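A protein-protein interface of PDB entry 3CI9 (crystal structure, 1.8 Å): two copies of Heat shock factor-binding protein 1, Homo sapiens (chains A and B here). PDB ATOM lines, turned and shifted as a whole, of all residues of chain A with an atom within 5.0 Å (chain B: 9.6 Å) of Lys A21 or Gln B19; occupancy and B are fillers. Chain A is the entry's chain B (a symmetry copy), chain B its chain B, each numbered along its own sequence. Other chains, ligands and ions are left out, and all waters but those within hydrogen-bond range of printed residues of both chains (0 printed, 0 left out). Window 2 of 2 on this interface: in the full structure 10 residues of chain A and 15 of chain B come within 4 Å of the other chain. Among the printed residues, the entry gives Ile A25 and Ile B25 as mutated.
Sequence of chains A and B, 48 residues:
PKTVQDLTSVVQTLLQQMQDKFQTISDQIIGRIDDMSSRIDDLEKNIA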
ATOM      1  N   GLN A  17       1.911  11.846 -31.762  1.00  0.00           N
ATOM      2  CA  GLN A  17       2.014  10.546 -32.400  1.00  0.00           C
ATOM      3  C   GLN A  17       2.943   9.720 -31.535  1.00  0.00           C
ATOM      4  O   GLN A  17       2.672   8.554 -31.262  1.00  0.00           O
ATOM      5  CB  GLN A  17       2.596  10.683 -33.809  1.00  0.00           C
ATOM      6  CG  GLN A  17       1.895  11.738 -34.648  1.00  0.00           C
ATOM      7  CD  GLN A  17       2.395  11.788 -36.077  1.00  0.00           C
ATOM      8  OE1 GLN A  17       3.600  11.706 -36.332  1.00  0.00           O
ATOM      9  NE2 GLN A  17       1.467  11.941 -37.019  1.00  0.00           N
ATOM     10  N   MET A  18       4.034  10.343 -31.095  1.00  0.00           N
ATOM     11  CA  MET A  18       5.019   9.680 -30.247  1.00  0.00           C
ATOM     12  C   MET A  18       4.380   9.218 -28.931  1.00  0.00           C
ATOM     13  O   MET A  18       4.766   8.189 -28.377  1.00  0.00           O
ATOM     14  CB  MET A  18       6.198  10.625 -29.969  1.00  0.00           C
ATOM     15  CG  MET A  18       7.281  10.043 -29.054  1.00  0.00           C
ATOM     16  SD  MET A  18       8.766  11.084 -28.863  1.00  0.00           S
ATOM     17  CE  MET A  18      10.007   9.863 -28.381  1.00  0.00           C
ATOM     18  N   GLN A  19       3.400   9.965 -28.431  1.00  0.00           N
ATOM     19  CA  GLN A  19       2.755   9.569 -27.194  1.00  0.00           C
ATOM     20  C   GLN A  19       1.674   8.517 -27.416  1.00  0.00           C
ATOM     21  O   GLN A  19       1.376   7.744 -26.512  1.00  0.00           O
ATOM     22  CB  GLN A  19       2.141  10.766 -26.491  1.00  0.00           C
ATOM     23  CG  GLN A  19       1.616  10.402 -25.115  1.00  0.00           C
ATOM     24  CD  GLN A  19       0.715  11.466 -24.536  1.00  0.00           C
ATOM     25  OE1 GLN A  19      -0.336  11.775 -25.096  1.00  0.00           O
ATOM     26  NE2 GLN A  19       1.120  12.036 -23.408  1.00  0.00           N
ATOM     27  N   ASP A  20       1.078   8.495 -28.606  1.00  0.00           N
ATOM     28  CA  ASP A  20       0.044   7.507 -28.924  1.00  0.00           C
ATOM     29  C   ASP A  20       0.687   6.130 -29.010  1.00  0.00           C
ATOM     30  O   ASP A  20       0.107   5.123 -28.587  1.00  0.00           O
ATOM     31  CB  ASP A  20      -0.628   7.816 -30.264  1.00  0.00           C
ATOM     32  CG  ASP A  20      -1.618   8.959 -30.172  1.00  0.00           C
ATOM     33  OD1 ASP A  20      -2.387   8.988 -29.184  1.00  0.00           O
ATOM     34  OD2 ASP A  20      -1.631   9.811 -31.095  1.00  0.00           O
ATOM     35  N   LYS A  21       1.886   6.103 -29.582  1.00  0.00           N
ATOM     36  CA  LYS A  21       2.655   4.877 -29.720  1.00  0.00           C
ATOM     37  C   LYS A  21       2.966   4.395 -28.302  1.00  0.00           C
ATOM     38  O   LYS A  21       2.887   3.208 -27.996  1.00  0.00           O
ATOM     39  CB  LYS A  21       3.945   5.161 -30.493  1.00  0.00           C
ATOM     40  CG  LYS A  21       4.757   3.933 -30.809  1.00  0.00           C
ATOM     41  CD  LYS A  21       5.991   4.288 -31.598  1.00  0.00           C
ATOM     42  CE  LYS A  21       6.855   3.057 -31.820  1.00  0.00           C
ATOM     43  NZ  LYS A  21       7.264   2.456 -30.516  1.00  0.00           N
ATOM     44  N   PHE A  22       3.317   5.342 -27.443  1.00  0.00           N
ATOM     45  CA  PHE A  22       3.614   5.074 -26.044  1.00  0.00           C
ATOM     46  C   PHE A  22       2.395   4.415 -25.384  1.00  0.00           C
ATOM     47  O   PHE A  22       2.504   3.361 -24.747  1.00  0.00           O
ATOM     48  CB  PHE A  22       3.941   6.405 -25.354  1.00  0.00           C
ATOM     49  CG  PHE A  22       3.853   6.368 -23.853  1.00  0.00           C
ATOM     50  CD1 PHE A  22       3.276   7.431 -23.160  1.00  0.00           C
ATOM     51  CD2 PHE A  22       4.360   5.292 -23.129  1.00  0.00           C
ATOM     52  CE1 PHE A  22       3.207   7.426 -21.771  1.00  0.00           C
ATOM     53  CE2 PHE A  22       4.297   5.275 -21.737  1.00  0.00           C
ATOM     54  CZ  PHE A  22       3.718   6.343 -21.058  1.00  0.00           C
ATOM     55  N   GLN A  23       1.238   5.057 -25.540  1.00  0.00           N
ATOM     56  CA  GLN A  23      -0.014   4.565 -24.977  1.00  0.00           C
ATOM     57  C   GLN A  23      -0.316   3.166 -25.479  1.00  0.00           C
ATOM     58  O   GLN A  23      -0.671   2.280 -24.703  1.00  0.00           O
ATOM     59  CB  GLN A  23      -1.170   5.489 -25.365  1.00  0.00           C
ATOM     60  CG  GLN A  23      -1.143   6.839 -24.678  1.00  0.00           C
ATOM     61  CD  GLN A  23      -1.071   6.719 -23.172  1.00  0.00           C
ATOM     62  OE1 GLN A  23      -1.843   5.979 -22.557  1.00  0.00           O
ATOM     63  NE2 GLN A  23      -0.142   7.451 -22.564  1.00  0.00           N
ATOM     64  N   THR A  24      -0.181   2.990 -26.789  1.00  0.00           N
ATOM     65  CA  THR A  24      -0.425   1.710 -27.445  1.00  0.00           C
ATOM     66  C   THR A  24       0.301   0.547 -26.766  1.00  0.00           C
ATOM     67  O   THR A  24      -0.311  -0.473 -26.441  1.00  0.00           O
ATOM     68  CB  THR A  24       0.004   1.779 -28.927  1.00  0.00           C
ATOM     69  OG1 THR A  24      -0.840   2.710 -29.619  1.00  0.00           O
ATOM     70  CG2 THR A  24      -0.086   0.404 -29.586  1.00  0.00           C
ATOM     71  N   ILE A  25       1.606   0.700 -26.560  1.00  0.00           N
ATOM     72  CA  ILE A  25       2.388  -0.343 -25.915  1.00  0.00           C
ATOM     73  C   ILE A  25       1.958  -0.467 -24.456  1.00  0.00           C
ATOM     74  O   ILE A  25       1.825  -1.568 -23.934  1.00  0.00           O
ATOM     75  CB  ILE A  25       3.910  -0.031 -25.986  1.00  0.00           C
ATOM     76  CG1 ILE A  25       4.355   0.039 -27.453  1.00  0.00           C
ATOM     77  CG2 ILE A  25       4.712  -1.097 -25.225  1.00  0.00           C
ATOM     78  CD1 ILE A  25       5.844   0.287 -27.649  1.00  0.00           C
ATOM     79  N   VAL B  11      16.158  17.352 -34.575  1.00  0.00           N
ATOM     80  CA  VAL B  11      14.836  17.141 -33.995  1.00  0.00           C
ATOM     81  C   VAL B  11      14.591  15.640 -34.050  1.00  0.00           C
ATOM     82  O   VAL B  11      14.086  15.025 -33.107  1.00  0.00           O
ATOM     83  CB  VAL B  11      13.746  17.834 -34.817  1.00  0.00           C
ATOM     84  CG1 VAL B  11      12.380  17.487 -34.259  1.00  0.00           C
ATOM     85  CG2 VAL B  11      13.972  19.332 -34.811  1.00  0.00           C
ATOM     86  N   GLN B  12      14.980  15.070 -35.182  1.00  0.00           N
ATOM     87  CA  GLN B  12      14.850  13.654 -35.461  1.00  0.00           C
ATOM     88  C   GLN B  12      15.617  12.824 -34.424  1.00  0.00           C
ATOM     89  O   GLN B  12      15.186  11.739 -34.041  1.00  0.00           O
ATOM     90  CB  GLN B  12      15.404  13.400 -36.855  1.00  0.00           C
ATOM     91  CG  GLN B  12      14.844  12.210 -37.573  1.00  0.00           C
ATOM     92  CD  GLN B  12      15.362  12.140 -38.990  1.00  0.00           C
ATOM     93  OE1 GLN B  12      16.570  12.094 -39.216  1.00  0.00           O
ATOM     94  NE2 GLN B  12      14.452  12.139 -39.955  1.00  0.00           N
ATOM     95  N   THR B  13      16.754  13.352 -33.980  1.00  0.00           N
ATOM     96  CA  THR B  13      17.603  12.689 -32.988  1.00  0.00           C
ATOM     97  C   THR B  13      16.997  12.836 -31.586  1.00  0.00           C
ATOM     98  O   THR B  13      16.697  11.844 -30.928  1.00  0.00           O
ATOM     99  CB  THR B  13      19.047  13.292 -32.991  1.00  0.00           C
ATOM    100  OG1 THR B  13      19.608  13.198 -34.310  1.00  0.00           O
ATOM    101  CG2 THR B  13      19.957  12.543 -32.017  1.00  0.00           C
ATOM    102  N   LEU B  14      16.815  14.072 -31.135  1.00  0.00           N
ATOM    103  CA  LEU B  14      16.247  14.310 -29.816  1.00  0.00           C
ATOM    104  C   LEU B  14      15.008  13.451 -29.596  1.00  0.00           C
ATOM    105  O   LEU B  14      14.764  12.967 -28.492  1.00  0.00           O
ATOM    106  CB  LEU B  14      15.870  15.789 -29.646  1.00  0.00           C
ATOM    107  CG  LEU B  14      16.951  16.859 -29.461  1.00  0.00           C
ATOM    108  CD1 LEU B  14      16.294  18.229 -29.355  1.00  0.00           C
ATOM    109  CD2 LEU B  14      17.758  16.573 -28.210  1.00  0.00           C
ATOM    110  N   LEU B  15      14.221  13.267 -30.648  1.00  0.00           N
ATOM    111  CA  LEU B  15      13.011  12.474 -30.522  1.00  0.00           C
ATOM    112  C   LEU B  15      13.296  10.976 -30.559  1.00  0.00           C
ATOM    113  O   LEU B  15      12.662  10.198 -29.838  1.00  0.00           O
ATOM    114  CB  LEU B  15      12.011  12.858 -31.619  1.00  0.00           C
ATOM    115  CG  LEU B  15      11.328  14.232 -31.505  1.00  0.00           C
ATOM    116  CD1 LEU B  15      10.433  14.443 -32.703  1.00  0.00           C
ATOM    117  CD2 LEU B  15      10.512  14.321 -30.226  1.00  0.00           C
ATOM    118  N   GLN B  16      14.261  10.576 -31.385  1.00  0.00           N
ATOM    119  CA  GLN B  16      14.627   9.165 -31.510  1.00  0.00           C
ATOM    120  C   GLN B  16      15.359   8.613 -30.299  1.00  0.00           C
ATOM    121  O   GLN B  16      15.514   7.404 -30.158  1.00  0.00           O
ATOM    122  CB  GLN B  16      15.477   8.939 -32.759  1.00  0.00           C
ATOM    123  CG  GLN B  16      14.766   8.087 -33.802  1.00  0.00           C
ATOM    124  CD  GLN B  16      15.544   7.982 -35.099  1.00  0.00           C
ATOM    125  OE1 GLN B  16      15.067   7.403 -36.082  1.00  0.00           O
ATOM    126  NE2 GLN B  16      16.752   8.546 -35.110  1.00  0.00           N
ATOM    127  N   GLN B  17      15.814   9.505 -29.428  1.00  0.00           N
ATOM    128  CA  GLN B  17      16.513   9.090 -28.225  1.00  0.00           C
ATOM    129  C   GLN B  17      15.452   8.902 -27.161  1.00  0.00           C
ATOM    130  O   GLN B  17      15.476   7.922 -26.421  1.00  0.00           O
ATOM    131  CB  GLN B  17      17.510  10.166 -27.784  1.00  0.00           C
ATOM    132  CG  GLN B  17      18.420  10.636 -28.906  1.00  0.00           C
ATOM    133  CD  GLN B  17      19.480  11.611 -28.439  1.00  0.00           C
ATOM    134  OE1 GLN B  17      19.208  12.514 -27.641  1.00  0.00           O
ATOM    135  NE2 GLN B  17      20.699  11.444 -28.949  1.00  0.00           N
ATOM    136  N   MET B  18      14.512   9.842 -27.105  1.00  0.00           N
ATOM    137  CA  MET B  18      13.422   9.793 -26.137  1.00  0.00           C
ATOM    138  C   MET B  18      12.575   8.530 -26.335  1.00  0.00           C
ATOM    139  O   MET B  18      12.050   7.972 -25.372  1.00  0.00           O
ATOM    140  CB  MET B  18      12.547  11.050 -26.264  1.00  0.00           C
ATOM    141  CG  MET B  18      11.344  11.089 -25.315  1.00  0.00           C
ATOM    142  SD  MET B  18      10.405  12.652 -25.330  1.00  0.00           S
ATOM    143  CE  MET B  18       9.606  12.612 -23.711  1.00  0.00           C
ATOM    144  N   GLN B  19      12.447   8.067 -27.575  1.00  0.00           N
ATOM    145  CA  GLN B  19      11.665   6.870 -27.818  1.00  0.00           C
ATOM    146  C   GLN B  19      12.461   5.596 -27.557  1.00  0.00           C
ATOM    147  O   GLN B  19      11.880   4.562 -27.247  1.00  0.00           O
ATOM    148  CB  GLN B  19      11.138   6.840 -29.240  1.00  0.00           C
ATOM    149  CG  GLN B  19      10.178   5.688 -29.462  1.00  0.00           C
ATOM    150  CD  GLN B  19       9.902   5.432 -30.924  1.00  0.00           C
ATOM    151  OE1 GLN B  19      10.810   5.109 -31.689  1.00  0.00           O
ATOM    152  NE2 GLN B  19       8.645   5.574 -31.324  1.00  0.00           N
ATOM    153  N   ASP B  20      13.783   5.663 -27.698  1.00  0.00           N
ATOM    154  CA  ASP B  20      14.638   4.499 -27.447  1.00  0.00           C
ATOM    155  C   ASP B  20      14.623   4.187 -25.958  1.00  0.00           C
ATOM    156  O   ASP B  20      14.622   3.021 -25.547  1.00  0.00           O
ATOM    157  CB  ASP B  20      16.083   4.767 -27.875  1.00  0.00           C
ATOM    158  CG  ASP B  20      16.271   4.699 -29.377  1.00  0.00           C
ATOM    159  OD1 ASP B  20      15.709   3.765 -29.993  1.00  0.00           O
ATOM    160  OD2 ASP B  20      16.991   5.568 -29.928  1.00  0.00           O
ATOM    161  N   LYS B  21      14.629   5.250 -25.161  1.00  0.00           N
ATOM    162  CA  LYS B  21      14.587   5.136 -23.712  1.00  0.00           C
ATOM    163  C   LYS B  21      13.247   4.483 -23.365  1.00  0.00           C
ATOM    164  O   LYS B  21      13.163   3.611 -22.502  1.00  0.00           O
ATOM    165  CB  LYS B  21      14.693   6.526 -23.080  1.00  0.00           C
ATOM    166  CG  LYS B  21      14.792   6.514 -21.579  1.00  0.00           C
ATOM    167  CD  LYS B  21      14.927   7.914 -21.034  1.00  0.00           C
ATOM    168  CE  LYS B  21      14.920   7.898 -19.513  1.00  0.00           C
ATOM    169  NZ  LYS B  21      13.658   7.291 -18.996  1.00  0.00           N
ATOM    170  N   PHE B  22      12.204   4.918 -24.057  1.00  0.00           N
ATOM    171  CA  PHE B  22      10.861   4.386 -23.887  1.00  0.00           C
ATOM    172  C   PHE B  22      10.874   2.876 -24.158  1.00  0.00           C
ATOM    173  O   PHE B  22      10.396   2.076 -23.345  1.00  0.00           O
ATOM    174  CB  PHE B  22       9.929   5.099 -24.876  1.00  0.00           C
ATOM    175  CG  PHE B  22       8.626   4.389 -25.129  1.00  0.00           C
ATOM    176  CD1 PHE B  22       8.112   4.312 -26.422  1.00  0.00           C
ATOM    177  CD2 PHE B  22       7.904   3.818 -24.084  1.00  0.00           C
ATOM    178  CE1 PHE B  22       6.898   3.681 -26.671  1.00  0.00           C
ATOM    179  CE2 PHE B  22       6.687   3.183 -24.322  1.00  0.00           C
ATOM    180  CZ  PHE B  22       6.184   3.113 -25.617  1.00  0.00           C
ATOM    181  N   GLN B  23      11.421   2.503 -25.314  1.00  0.00           N
ATOM    182  CA  GLN B  23      11.515   1.107 -25.724  1.00  0.00           C
ATOM    183  C   GLN B  23      12.276   0.294 -24.695  1.00  0.00           C
ATOM    184  O   GLN B  23      11.849  -0.792 -24.305  1.00  0.00           O
ATOM    185  CB  GLN B  23      12.232   0.994 -27.070  1.00  0.00           C
ATOM    186  CG  GLN B  23      11.427   1.509 -28.248  1.00  0.00           C
ATOM    187  CD  GLN B  23      10.064   0.861 -28.342  1.00  0.00           C
ATOM    188  OE1 GLN B  23       9.939  -0.365 -28.284  1.00  0.00           O
ATOM    189  NE2 GLN B  23       9.029   1.682 -28.491  1.00  0.00           N
ATOM    190  N   THR B  24      13.415   0.833 -24.273  1.00  0.00           N
ATOM    191  CA  THR B  24      14.275   0.195 -23.283  1.00  0.00           C
ATOM    192  C   THR B  24      13.511  -0.255 -22.035  1.00  0.00           C
ATOM    193  O   THR B  24      13.615  -1.410 -21.616  1.00  0.00           O
ATOM    194  CB  THR B  24      15.411   1.154 -22.863  1.00  0.00           C
ATOM    195  OG1 THR B  24      16.267   1.391 -23.989  1.00  0.00           O
ATOM    196  CG2 THR B  24      16.220   0.569 -21.707  1.00  0.00           C
ATOM    197  N   ILE B  25      12.752   0.662 -21.442  1.00  0.00           N
ATOM    198  CA  ILE B  25      11.978   0.336 -20.253  1.00  0.00           C
ATOM    199  C   ILE B  25      10.871  -0.646 -20.625  1.00  0.00           C
ATOM    200  O   ILE B  25      10.605  -1.595 -19.896  1.00  0.00           O
ATOM    201  CB  ILE B  25      11.354   1.612 -19.619  1.00  0.00           C
ATOM    202  CG1 ILE B  25      12.470   2.576 -19.194  1.00  0.00           C
ATOM    203  CG2 ILE B  25      10.472   1.237 -18.419  1.00  0.00           C
ATOM    204  CD1 ILE B  25      11.979   3.844 -18.510  1.00  0.00           C
ATOM    205  N   SER B  26      10.238  -0.422 -21.767  1.00  0.00           N
ATOM    206  CA  SER B  26       9.164  -1.293 -22.208  1.00  0.00           C
ATOM    207  C   SER B  26       9.661  -2.713 -22.428  1.00  0.00           C
ATOM    208  O   SER B  26       9.188  -3.645 -21.778  1.00  0.00           O
ATOM    209  CB  SER B  26       8.548  -0.758 -23.497  1.00  0.00           C
ATOM    210  OG  SER B  26       8.059   0.557 -23.308  1.00  0.00           O
ATOM    211  N   ASP B  27      10.608  -2.879 -23.350  1.00  0.00           N
ATOM    212  CA  ASP B  27      11.168  -4.192 -23.651  1.00  0.00           C
ATOM    213  C   ASP B  27      11.603  -4.886 -22.365  1.00  0.00           C
ATOM    214  O   ASP B  27      11.548  -6.109 -22.236  1.00  0.00           O
ATOM    215  CB  ASP B  27      12.368  -4.054 -24.598  1.00  0.00           C
ATOM    216  CG  ASP B  27      11.957  -3.684 -26.018  1.00  0.00           C
ATOM    217  OD1 ASP B  27      11.098  -4.386 -26.586  1.00  0.00           O
ATOM    218  OD2 ASP B  27      12.491  -2.699 -26.576  1.00  0.00           O
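Among the printed residues, merely in contact across the chains: Met A18 with Leu B15, Met A18 with Met B18, Met A18 with Gln B19, Lys A21 with Gln B19, Phe A22 with Phe B22, Ile A25 with Phe B22 and Ile A25 with Gln B23.
NE2 of Gln B23 sits close to NZ of Lys A21, at 2.8 Å.
Of the 9 printed residues of chain A, 4 touch a printed residue of chain B. Printed residues of chain A that touch a printed residue of chain B: Met A18, Lys A21, Phe A22 and Ile A25. Hydrophobic or aromatic side chains of chain A within 4 Å of the printed part of chain B: Met A18, Phe A22 and Ile A25. Along chain A the printed residues that touch a printed residue of chain B span positions 18 to 25. Of the 17 printed residues of chain B, 5 touch a printed residue of chain A. Printed residues of chain B that touch a printed residue of chain A: Leu B15, Met B18, Gln B19, Phe B22 and Gln B23. Among the printed residues, 8 pairs touch across the chains. Among the printed residues, no Asp or Glu carboxylate lies within 4 Å of a Lys or Arg side-chain nitrogen of the other chain.
Lys A21 touches just these residues of chain B: Gln B19 and Gln B23. Gln B19 touches just these residues of chain A: Met A18 (3.1 Å) and Lys A21 (3.0 Å). Of the printed residues of chain B, Ile A25 touches Phe B22 (3.5 Å) and Gln B23 (3.6 Å). Printed residues of chain B within 4 Å of Met A18: Leu B15 (3.0 Å), Met B18 (3.5 Å) and Gln B19 (3.1 Å). Of the printed residues of chain A, Phe B22 touches Phe A22 (3.3 Å) and Ile A25 (3.5 Å). Of the printed residues of chain A, Gln B23 touches Lys A21 and Ile A25. Printed residues of chain B within 4 Å of Phe A22: Phe B22 (3.3 Å). Lys B21 touches none of the printed residues of chain A. The nearest printed residue of chain A that does not touch Gln B19 is Phe A22 (6.6 Å).
The backbone carbonyl oxygen (O) of Phe B22 lies within hydrogen-bond range of the side-chain hydroxyl (OG) of Ser B26 (2.8 Å).
Lys A21 touches Gln B19, but with the chains exchanged Gln A19 does not touch Lys B21 (12.3 Å). Lys A21 touches Gln B23, but with the chains exchanged Gln A23 does not touch Lys B21 (12.2 Å). Phe A22 touches its own counterpart, Phe B22. Ile A25 touches Gln B23, but with the chains exchanged Gln A23 does not touch Ile B25 (12.2 Å). 9 positions are printed for both chains. Of the 8 pairs that touch across the chains among the printed residues, 2 have their exchanged pair printed and touching as well.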
